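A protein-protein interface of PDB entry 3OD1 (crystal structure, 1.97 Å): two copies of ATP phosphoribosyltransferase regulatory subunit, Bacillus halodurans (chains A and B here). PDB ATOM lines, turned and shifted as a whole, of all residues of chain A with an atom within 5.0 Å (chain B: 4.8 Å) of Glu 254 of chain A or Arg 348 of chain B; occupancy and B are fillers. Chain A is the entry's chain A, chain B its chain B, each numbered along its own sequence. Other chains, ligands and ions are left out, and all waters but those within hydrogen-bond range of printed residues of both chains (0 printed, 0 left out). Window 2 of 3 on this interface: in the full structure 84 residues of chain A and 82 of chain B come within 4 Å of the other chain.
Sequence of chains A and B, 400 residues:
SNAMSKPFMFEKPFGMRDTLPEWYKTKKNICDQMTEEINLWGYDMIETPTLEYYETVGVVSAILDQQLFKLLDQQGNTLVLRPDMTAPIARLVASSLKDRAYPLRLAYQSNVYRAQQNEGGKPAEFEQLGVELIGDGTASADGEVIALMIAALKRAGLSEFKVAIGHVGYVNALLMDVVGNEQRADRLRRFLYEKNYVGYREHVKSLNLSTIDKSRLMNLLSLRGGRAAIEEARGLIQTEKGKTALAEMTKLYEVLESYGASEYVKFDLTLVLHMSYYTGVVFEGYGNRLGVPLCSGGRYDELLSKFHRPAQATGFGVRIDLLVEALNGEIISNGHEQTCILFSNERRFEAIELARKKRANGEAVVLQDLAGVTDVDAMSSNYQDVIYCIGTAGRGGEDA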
ATOM      1  N   SER A 140       5.699  18.841  19.931  1.00  0.00           N
ATOM      2  CA  SER A 140       4.797  18.821  21.079  1.00  0.00           C
ATOM      3  C   SER A 140       4.187  20.202  21.250  1.00  0.00           C
ATOM      4  O   SER A 140       3.023  20.349  21.655  1.00  0.00           O
ATOM      5  CB  SER A 140       5.541  18.428  22.358  1.00  0.00           C
ATOM      6  OG  SER A 140       5.897  17.057  22.329  1.00  0.00           O
ATOM      7  N   ARG A 227      -2.988   9.857   8.014  1.00  0.00           N
ATOM      8  CA  ARG A 227      -1.773   9.069   7.933  1.00  0.00           C
ATOM      9  C   ARG A 227      -1.442   8.665   6.499  1.00  0.00           C
ATOM     10  O   ARG A 227      -0.275   8.569   6.140  1.00  0.00           O
ATOM     11  CB  ARG A 227      -1.871   7.834   8.837  1.00  0.00           C
ATOM     12  CG  ARG A 227      -1.849   8.224  10.322  1.00  0.00           C
ATOM     13  CD  ARG A 227      -2.192   7.051  11.227  1.00  0.00           C
ATOM     14  NE  ARG A 227      -1.889   7.351  12.621  1.00  0.00           N
ATOM     15  CZ  ARG A 227      -0.679   7.199  13.152  1.00  0.00           C
ATOM     16  NH1 ARG A 227       0.312   6.747  12.397  1.00  0.00           N
ATOM     17  NH2 ARG A 227      -0.462   7.483  14.433  1.00  0.00           N
ATOM     18  N   THR A 250       4.665  13.795  11.153  1.00  0.00           N
ATOM     19  CA  THR A 250       4.326  12.496  11.751  1.00  0.00           C
ATOM     20  C   THR A 250       4.162  12.626  13.263  1.00  0.00           C
ATOM     21  O   THR A 250       3.183  12.158  13.843  1.00  0.00           O
ATOM     22  CB  THR A 250       5.419  11.444  11.431  1.00  0.00           C
ATOM     23  OG1 THR A 250       5.615  11.376  10.013  1.00  0.00           O
ATOM     24  CG2 THR A 250       5.034  10.048  11.961  1.00  0.00           C
ATOM     25  N   LYS A 251       5.126  13.267  13.904  1.00  0.00           N
ATOM     26  CA  LYS A 251       5.047  13.490  15.349  1.00  0.00           C
ATOM     27  C   LYS A 251       3.817  14.320  15.739  1.00  0.00           C
ATOM     28  O   LYS A 251       3.105  14.000  16.691  1.00  0.00           O
ATOM     29  CB  LYS A 251       6.319  14.172  15.840  1.00  0.00           C
ATOM     30  CG  LYS A 251       6.428  14.280  17.355  1.00  0.00           C
ATOM     31  CD  LYS A 251       7.455  13.301  17.916  1.00  0.00           C
ATOM     32  CE  LYS A 251       6.894  11.885  18.032  1.00  0.00           C
ATOM     33  NZ  LYS A 251       7.904  10.920  18.572  1.00  0.00           N
ATOM     34  N   LEU A 252       3.567  15.390  14.993  1.00  0.00           N
ATOM     35  CA  LEU A 252       2.405  16.242  15.254  1.00  0.00           C
ATOM     36  C   LEU A 252       1.085  15.479  15.205  1.00  0.00           C
ATOM     37  O   LEU A 252       0.213  15.646  16.061  1.00  0.00           O
ATOM     38  CB  LEU A 252       2.371  17.390  14.236  1.00  0.00           C
ATOM     39  CG  LEU A 252       1.115  18.238  14.237  1.00  0.00           C
ATOM     40  CD1 LEU A 252       0.964  18.940  15.600  1.00  0.00           C
ATOM     41  CD2 LEU A 252       1.198  19.253  13.099  1.00  0.00           C
ATOM     42  N   TYR A 253       0.924  14.650  14.186  1.00  0.00           N
ATOM     43  CA  TYR A 253      -0.307  13.884  14.053  1.00  0.00           C
ATOM     44  C   TYR A 253      -0.470  12.965  15.273  1.00  0.00           C
ATOM     45  O   TYR A 253      -1.566  12.792  15.785  1.00  0.00           O
ATOM     46  CB  TYR A 253      -0.279  13.059  12.758  1.00  0.00           C
ATOM     47  CG  TYR A 253      -1.631  12.562  12.312  1.00  0.00           C
ATOM     48  CD1 TYR A 253      -2.467  13.362  11.548  1.00  0.00           C
ATOM     49  CD2 TYR A 253      -2.072  11.296  12.651  1.00  0.00           C
ATOM     50  CE1 TYR A 253      -3.687  12.911  11.130  1.00  0.00           C
ATOM     51  CE2 TYR A 253      -3.310  10.850  12.252  1.00  0.00           C
ATOM     52  CZ  TYR A 253      -4.105  11.653  11.497  1.00  0.00           C
ATOM     53  OH  TYR A 253      -5.324  11.217  11.074  1.00  0.00           O
ATOM     54  N   GLU A 254       0.629  12.365  15.723  1.00  0.00           N
ATOM     55  CA  GLU A 254       0.584  11.479  16.882  1.00  0.00           C
ATOM     56  C   GLU A 254       0.232  12.247  18.154  1.00  0.00           C
ATOM     57  O   GLU A 254      -0.625  11.823  18.929  1.00  0.00           O
ATOM     58  CB  GLU A 254       1.927  10.781  17.062  1.00  0.00           C
ATOM     59  CG  GLU A 254       2.112   9.620  16.114  1.00  0.00           C
ATOM     60  CD  GLU A 254       3.543   9.132  16.079  1.00  0.00           C
ATOM     61  OE1 GLU A 254       4.390   9.708  16.800  1.00  0.00           O
ATOM     62  OE2 GLU A 254       3.815   8.177  15.320  1.00  0.00           O
ATOM     63  N   VAL A 255       0.901  13.379  18.367  1.00  0.00           N
ATOM     64  CA  VAL A 255       0.561  14.245  19.495  1.00  0.00           C
ATOM     65  C   VAL A 255      -0.928  14.595  19.497  1.00  0.00           C
ATOM     66  O   VAL A 255      -1.588  14.507  20.538  1.00  0.00           O
ATOM     67  CB  VAL A 255       1.422  15.536  19.514  1.00  0.00           C
ATOM     68  CG1 VAL A 255       0.950  16.474  20.609  1.00  0.00           C
ATOM     69  CG2 VAL A 255       2.884  15.178  19.752  1.00  0.00           C
ATOM     70  N   LEU A 256      -1.462  14.993  18.341  1.00  0.00           N
ATOM     71  CA  LEU A 256      -2.884  15.359  18.249  1.00  0.00           C
ATOM     72  C   LEU A 256      -3.786  14.173  18.531  1.00  0.00           C
ATOM     73  O   LEU A 256      -4.854  14.333  19.119  1.00  0.00           O
ATOM     74  CB  LEU A 256      -3.231  15.996  16.893  1.00  0.00           C
ATOM     75  CG  LEU A 256      -2.674  17.414  16.660  1.00  0.00           C
ATOM     76  CD1 LEU A 256      -2.838  17.827  15.210  1.00  0.00           C
ATOM     77  CD2 LEU A 256      -3.334  18.440  17.595  1.00  0.00           C
ATOM     78  N   GLU A 257      -3.359  12.980  18.119  1.00  0.00           N
ATOM     79  CA  GLU A 257      -4.068  11.765  18.511  1.00  0.00           C
ATOM     80  C   GLU A 257      -4.065  11.592  20.020  1.00  0.00           C
ATOM     81  O   GLU A 257      -5.101  11.306  20.609  1.00  0.00           O
ATOM     82  CB  GLU A 257      -3.492  10.520  17.831  1.00  0.00           C
ATOM     83  CG  GLU A 257      -3.932  10.387  16.381  1.00  0.00           C
ATOM     84  CD  GLU A 257      -3.314   9.188  15.694  1.00  0.00           C
ATOM     85  OE1 GLU A 257      -2.197   8.797  16.084  1.00  0.00           O
ATOM     86  OE2 GLU A 257      -3.930   8.662  14.747  1.00  0.00           O
ATOM     87  N   SER A 258      -2.906  11.787  20.638  1.00  0.00           N
ATOM     88  CA  SER A 258      -2.789  11.711  22.090  1.00  0.00           C
ATOM     89  C   SER A 258      -3.678  12.707  22.809  1.00  0.00           C
ATOM     90  O   SER A 258      -4.165  12.409  23.898  1.00  0.00           O
ATOM     91  CB  SER A 258      -1.343  11.927  22.538  1.00  0.00           C
ATOM     92  OG  SER A 258      -0.506  10.890  22.074  1.00  0.00           O
ATOM     93  N   PHE B 343       7.560  16.236  30.428  1.00  0.00           N
ATOM     94  CA  PHE B 343       7.507  14.876  29.915  1.00  0.00           C
ATOM     95  C   PHE B 343       8.543  14.598  28.848  1.00  0.00           C
ATOM     96  O   PHE B 343       9.082  15.515  28.243  1.00  0.00           O
ATOM     97  CB  PHE B 343       6.103  14.522  29.407  1.00  0.00           C
ATOM     98  CG  PHE B 343       5.678  15.284  28.179  1.00  0.00           C
ATOM     99  CD1 PHE B 343       5.809  14.726  26.918  1.00  0.00           C
ATOM    100  CD2 PHE B 343       5.120  16.545  28.287  1.00  0.00           C
ATOM    101  CE1 PHE B 343       5.407  15.424  25.789  1.00  0.00           C
ATOM    102  CE2 PHE B 343       4.720  17.251  27.157  1.00  0.00           C
ATOM    103  CZ  PHE B 343       4.862  16.686  25.912  1.00  0.00           C
ATOM    104  N   SER B 344       8.839  13.318  28.648  1.00  0.00           N
ATOM    105  CA  SER B 344       9.599  12.884  27.480  1.00  0.00           C
ATOM    106  C   SER B 344       8.698  12.042  26.584  1.00  0.00           C
ATOM    107  O   SER B 344       7.552  11.742  26.937  1.00  0.00           O
ATOM    108  CB  SER B 344      10.847  12.103  27.877  1.00  0.00           C
ATOM    109  OG  SER B 344      10.510  10.903  28.551  1.00  0.00           O
ATOM    110  N   ASN B 345       9.227  11.659  25.430  1.00  0.00           N
ATOM    111  CA  ASN B 345       8.431  11.041  24.381  1.00  0.00           C
ATOM    112  C   ASN B 345       7.624   9.848  24.864  1.00  0.00           C
ATOM    113  O   ASN B 345       6.417   9.772  24.633  1.00  0.00           O
ATOM    114  CB  ASN B 345       9.336  10.620  23.226  1.00  0.00           C
ATOM    115  CG  ASN B 345       8.600  10.547  21.912  1.00  0.00           C
ATOM    116  OD1 ASN B 345       7.691  11.338  21.653  1.00  0.00           O
ATOM    117  ND2 ASN B 345       8.992   9.599  21.067  1.00  0.00           N
ATOM    118  N   GLU B 346       8.294   8.935  25.556  1.00  0.00           N
ATOM    119  CA  GLU B 346       7.701   7.654  25.927  1.00  0.00           C
ATOM    120  C   GLU B 346       6.548   7.761  26.911  1.00  0.00           C
ATOM    121  O   GLU B 346       5.682   6.892  26.940  1.00  0.00           O
ATOM    122  CB  GLU B 346       8.770   6.700  26.464  1.00  0.00           C
ATOM    123  CG  GLU B 346       9.795   6.301  25.426  1.00  0.00           C
ATOM    124  CD  GLU B 346      10.923   5.474  26.008  1.00  0.00           C
ATOM    125  OE1 GLU B 346      11.933   5.265  25.301  1.00  0.00           O
ATOM    126  OE2 GLU B 346      10.801   5.037  27.174  1.00  0.00           O
ATOM    127  N   ARG B 347       6.528   8.817  27.716  1.00  0.00           N
ATOM    128  CA  ARG B 347       5.435   8.996  28.672  1.00  0.00           C
ATOM    129  C   ARG B 347       4.501  10.161  28.316  1.00  0.00           C
ATOM    130  O   ARG B 347       3.813  10.698  29.184  1.00  0.00           O
ATOM    131  CB  ARG B 347       5.980   9.156  30.096  1.00  0.00           C
ATOM    132  CG  ARG B 347       6.761   7.952  30.582  1.00  0.00           C
ATOM    133  CD  ARG B 347       7.440   8.224  31.908  1.00  0.00           C
ATOM    134  NE  ARG B 347       6.497   8.251  33.024  1.00  0.00           N
ATOM    135  CZ  ARG B 347       6.858   8.378  34.299  1.00  0.00           C
ATOM    136  NH1 ARG B 347       8.142   8.486  34.618  1.00  0.00           N
ATOM    137  NH2 ARG B 347       5.941   8.392  35.256  1.00  0.00           N
ATOM    138  N   ARG B 348       4.478  10.541  27.041  1.00  0.00           N
ATOM    139  CA  ARG B 348       3.633  11.644  26.586  1.00  0.00           C
ATOM    140  C   ARG B 348       2.143  11.383  26.810  1.00  0.00           C
ATOM    141  O   ARG B 348       1.397  12.275  27.225  1.00  0.00           O
ATOM    142  CB  ARG B 348       3.885  11.959  25.105  1.00  0.00           C
ATOM    143  CG  ARG B 348       2.958  13.055  24.573  1.00  0.00           C
ATOM    144  CD  ARG B 348       3.182  13.354  23.104  1.00  0.00           C
ATOM    145  NE  ARG B 348       2.943  12.183  22.267  1.00  0.00           N
ATOM    146  CZ  ARG B 348       3.816  11.719  21.376  1.00  0.00           C
ATOM    147  NH1 ARG B 348       4.979  12.337  21.209  1.00  0.00           N
ATOM    148  NH2 ARG B 348       3.527  10.642  20.652  1.00  0.00           N
ATOM    149  N   PHE B 349       1.698  10.165  26.533  1.00  0.00           N
ATOM    150  CA  PHE B 349       0.283   9.880  26.705  1.00  0.00           C
ATOM    151  C   PHE B 349      -0.069   9.988  28.179  1.00  0.00           C
ATOM    152  O   PHE B 349      -1.080  10.583  28.544  1.00  0.00           O
ATOM    153  CB  PHE B 349      -0.084   8.502  26.156  1.00  0.00           C
ATOM    154  CG  PHE B 349      -1.564   8.258  26.110  1.00  0.00           C
ATOM    155  CD1 PHE B 349      -2.374   9.017  25.271  1.00  0.00           C
ATOM    156  CD2 PHE B 349      -2.150   7.283  26.913  1.00  0.00           C
ATOM    157  CE1 PHE B 349      -3.741   8.808  25.226  1.00  0.00           C
ATOM    158  CE2 PHE B 349      -3.517   7.065  26.876  1.00  0.00           C
ATOM    159  CZ  PHE B 349      -4.316   7.830  26.028  1.00  0.00           C
ATOM    160  N   GLU B 350       0.786   9.425  29.025  1.00  0.00           N
ATOM    161  CA  GLU B 350       0.587   9.501  30.465  1.00  0.00           C
ATOM    162  C   GLU B 350       0.482  10.939  30.955  1.00  0.00           C
ATOM    163  O   GLU B 350      -0.419  11.278  31.725  1.00  0.00           O
ATOM    164  CB  GLU B 350       1.714   8.781  31.208  1.00  0.00           C
ATOM    165  CG  GLU B 350       1.692   9.018  32.713  1.00  0.00           C
ATOM    166  CD  GLU B 350       2.920   8.462  33.401  1.00  0.00           C
ATOM    167  OE1 GLU B 350       3.602   7.612  32.788  1.00  0.00           O
ATOM    168  OE2 GLU B 350       3.199   8.875  34.550  1.00  0.00           O
ATOM    169  N   ALA B 351       1.410  11.784  30.522  1.00  0.00           N
ATOM    170  CA  ALA B 351       1.415  13.181  30.962  1.00  0.00           C
ATOM    171  C   ALA B 351       0.198  13.959  30.466  1.00  0.00           C
ATOM    172  O   ALA B 351      -0.392  14.750  31.210  1.00  0.00           O
ATOM    173  CB  ALA B 351       2.706  13.876  30.533  1.00  0.00           C
ATOM    174  N   ILE B 352      -0.161  13.763  29.205  1.00  0.00           N
ATOM    175  CA  ILE B 352      -1.351  14.410  28.665  1.00  0.00           C
ATOM    176  C   ILE B 352      -2.580  14.038  29.501  1.00  0.00           C
ATOM    177  O   ILE B 352      -3.355  14.905  29.904  1.00  0.00           O
ATOM    178  CB  ILE B 352      -1.584  14.058  27.179  1.00  0.00           C
ATOM    179  CG1 ILE B 352      -0.607  14.841  26.295  1.00  0.00           C
ATOM    180  CG2 ILE B 352      -3.042  14.362  26.780  1.00  0.00           C
ATOM    181  CD1 ILE B 352      -0.596  14.429  24.847  1.00  0.00           C
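Among the printed residues, pairs that only touch across the chains: Ser 140 of chain A with Phe 343 of chain B (3.7 Å), Lys 251 of chain A with Arg 348 of chain B (3.7 Å), Glu 254 of chain A with Arg 348 of chain B (3.9 Å), Val 255 of chain A with Arg 348 of chain B (3.8 Å), Ser 258 of chain A with Arg 348 of chain B (3.7 Å), Ser 258 of chain A with Phe 349 of chain B (3.9 Å) and Ser 258 of chain A with Ile 352 of chain B (3.5 Å).
O of Glu 254 of chain A is in hydrogen-bond range of OG of Ser 258 of chain A, at 3.3 Å. OD1 of Asn 345 of chain B is in hydrogen-bond range of NH1 of Arg 348 of chain B.
No position is printed for both chains.
Of the 11 printed residues of chain A, 5 touch a printed residue of chain B. Printed residues of chain A that touch a printed residue of chain B: Ser 140, Lys 251, Glu 254, Val 255 and Ser 258. Of the 10 printed residues of chain B, 5 touch a printed residue of chain A. Printed residues of chain B that touch a printed residue of chain A: Phe 343, Asn 345, Arg 348, Phe 349 and Ile 352. Hydrophobic or aromatic side chains of chain B that line the printed part of chain A: Phe 343, Phe 349 and Ile 352. Among the printed residues, no Asp or Glu carboxylate lies within 4 Å of a Lys or Arg side-chain nitrogen of the other chain.
The side-chain amide nitrogen (ND2) of Asn 345 of chain B lies close to the side-chain amino group (NZ) of Lys 251 of chain A (3.0 Å).
Glu 254 of chain A touches one residue of chain B. Of chain A, only Lys 251, Glu 254, Val 255 and Ser 258 come within 4 Å of Arg 348 of chain B. Of the printed residues of chain B, Ser 140 of chain A touches Phe 343 (3.7 Å). Of the printed residues of chain A, Phe 349 of chain B touches Ser 258 (3.9 Å). The nearest residue of chain A that does not touch Arg 348 of chain B is Ser 140 of chain A (4.7 Å).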
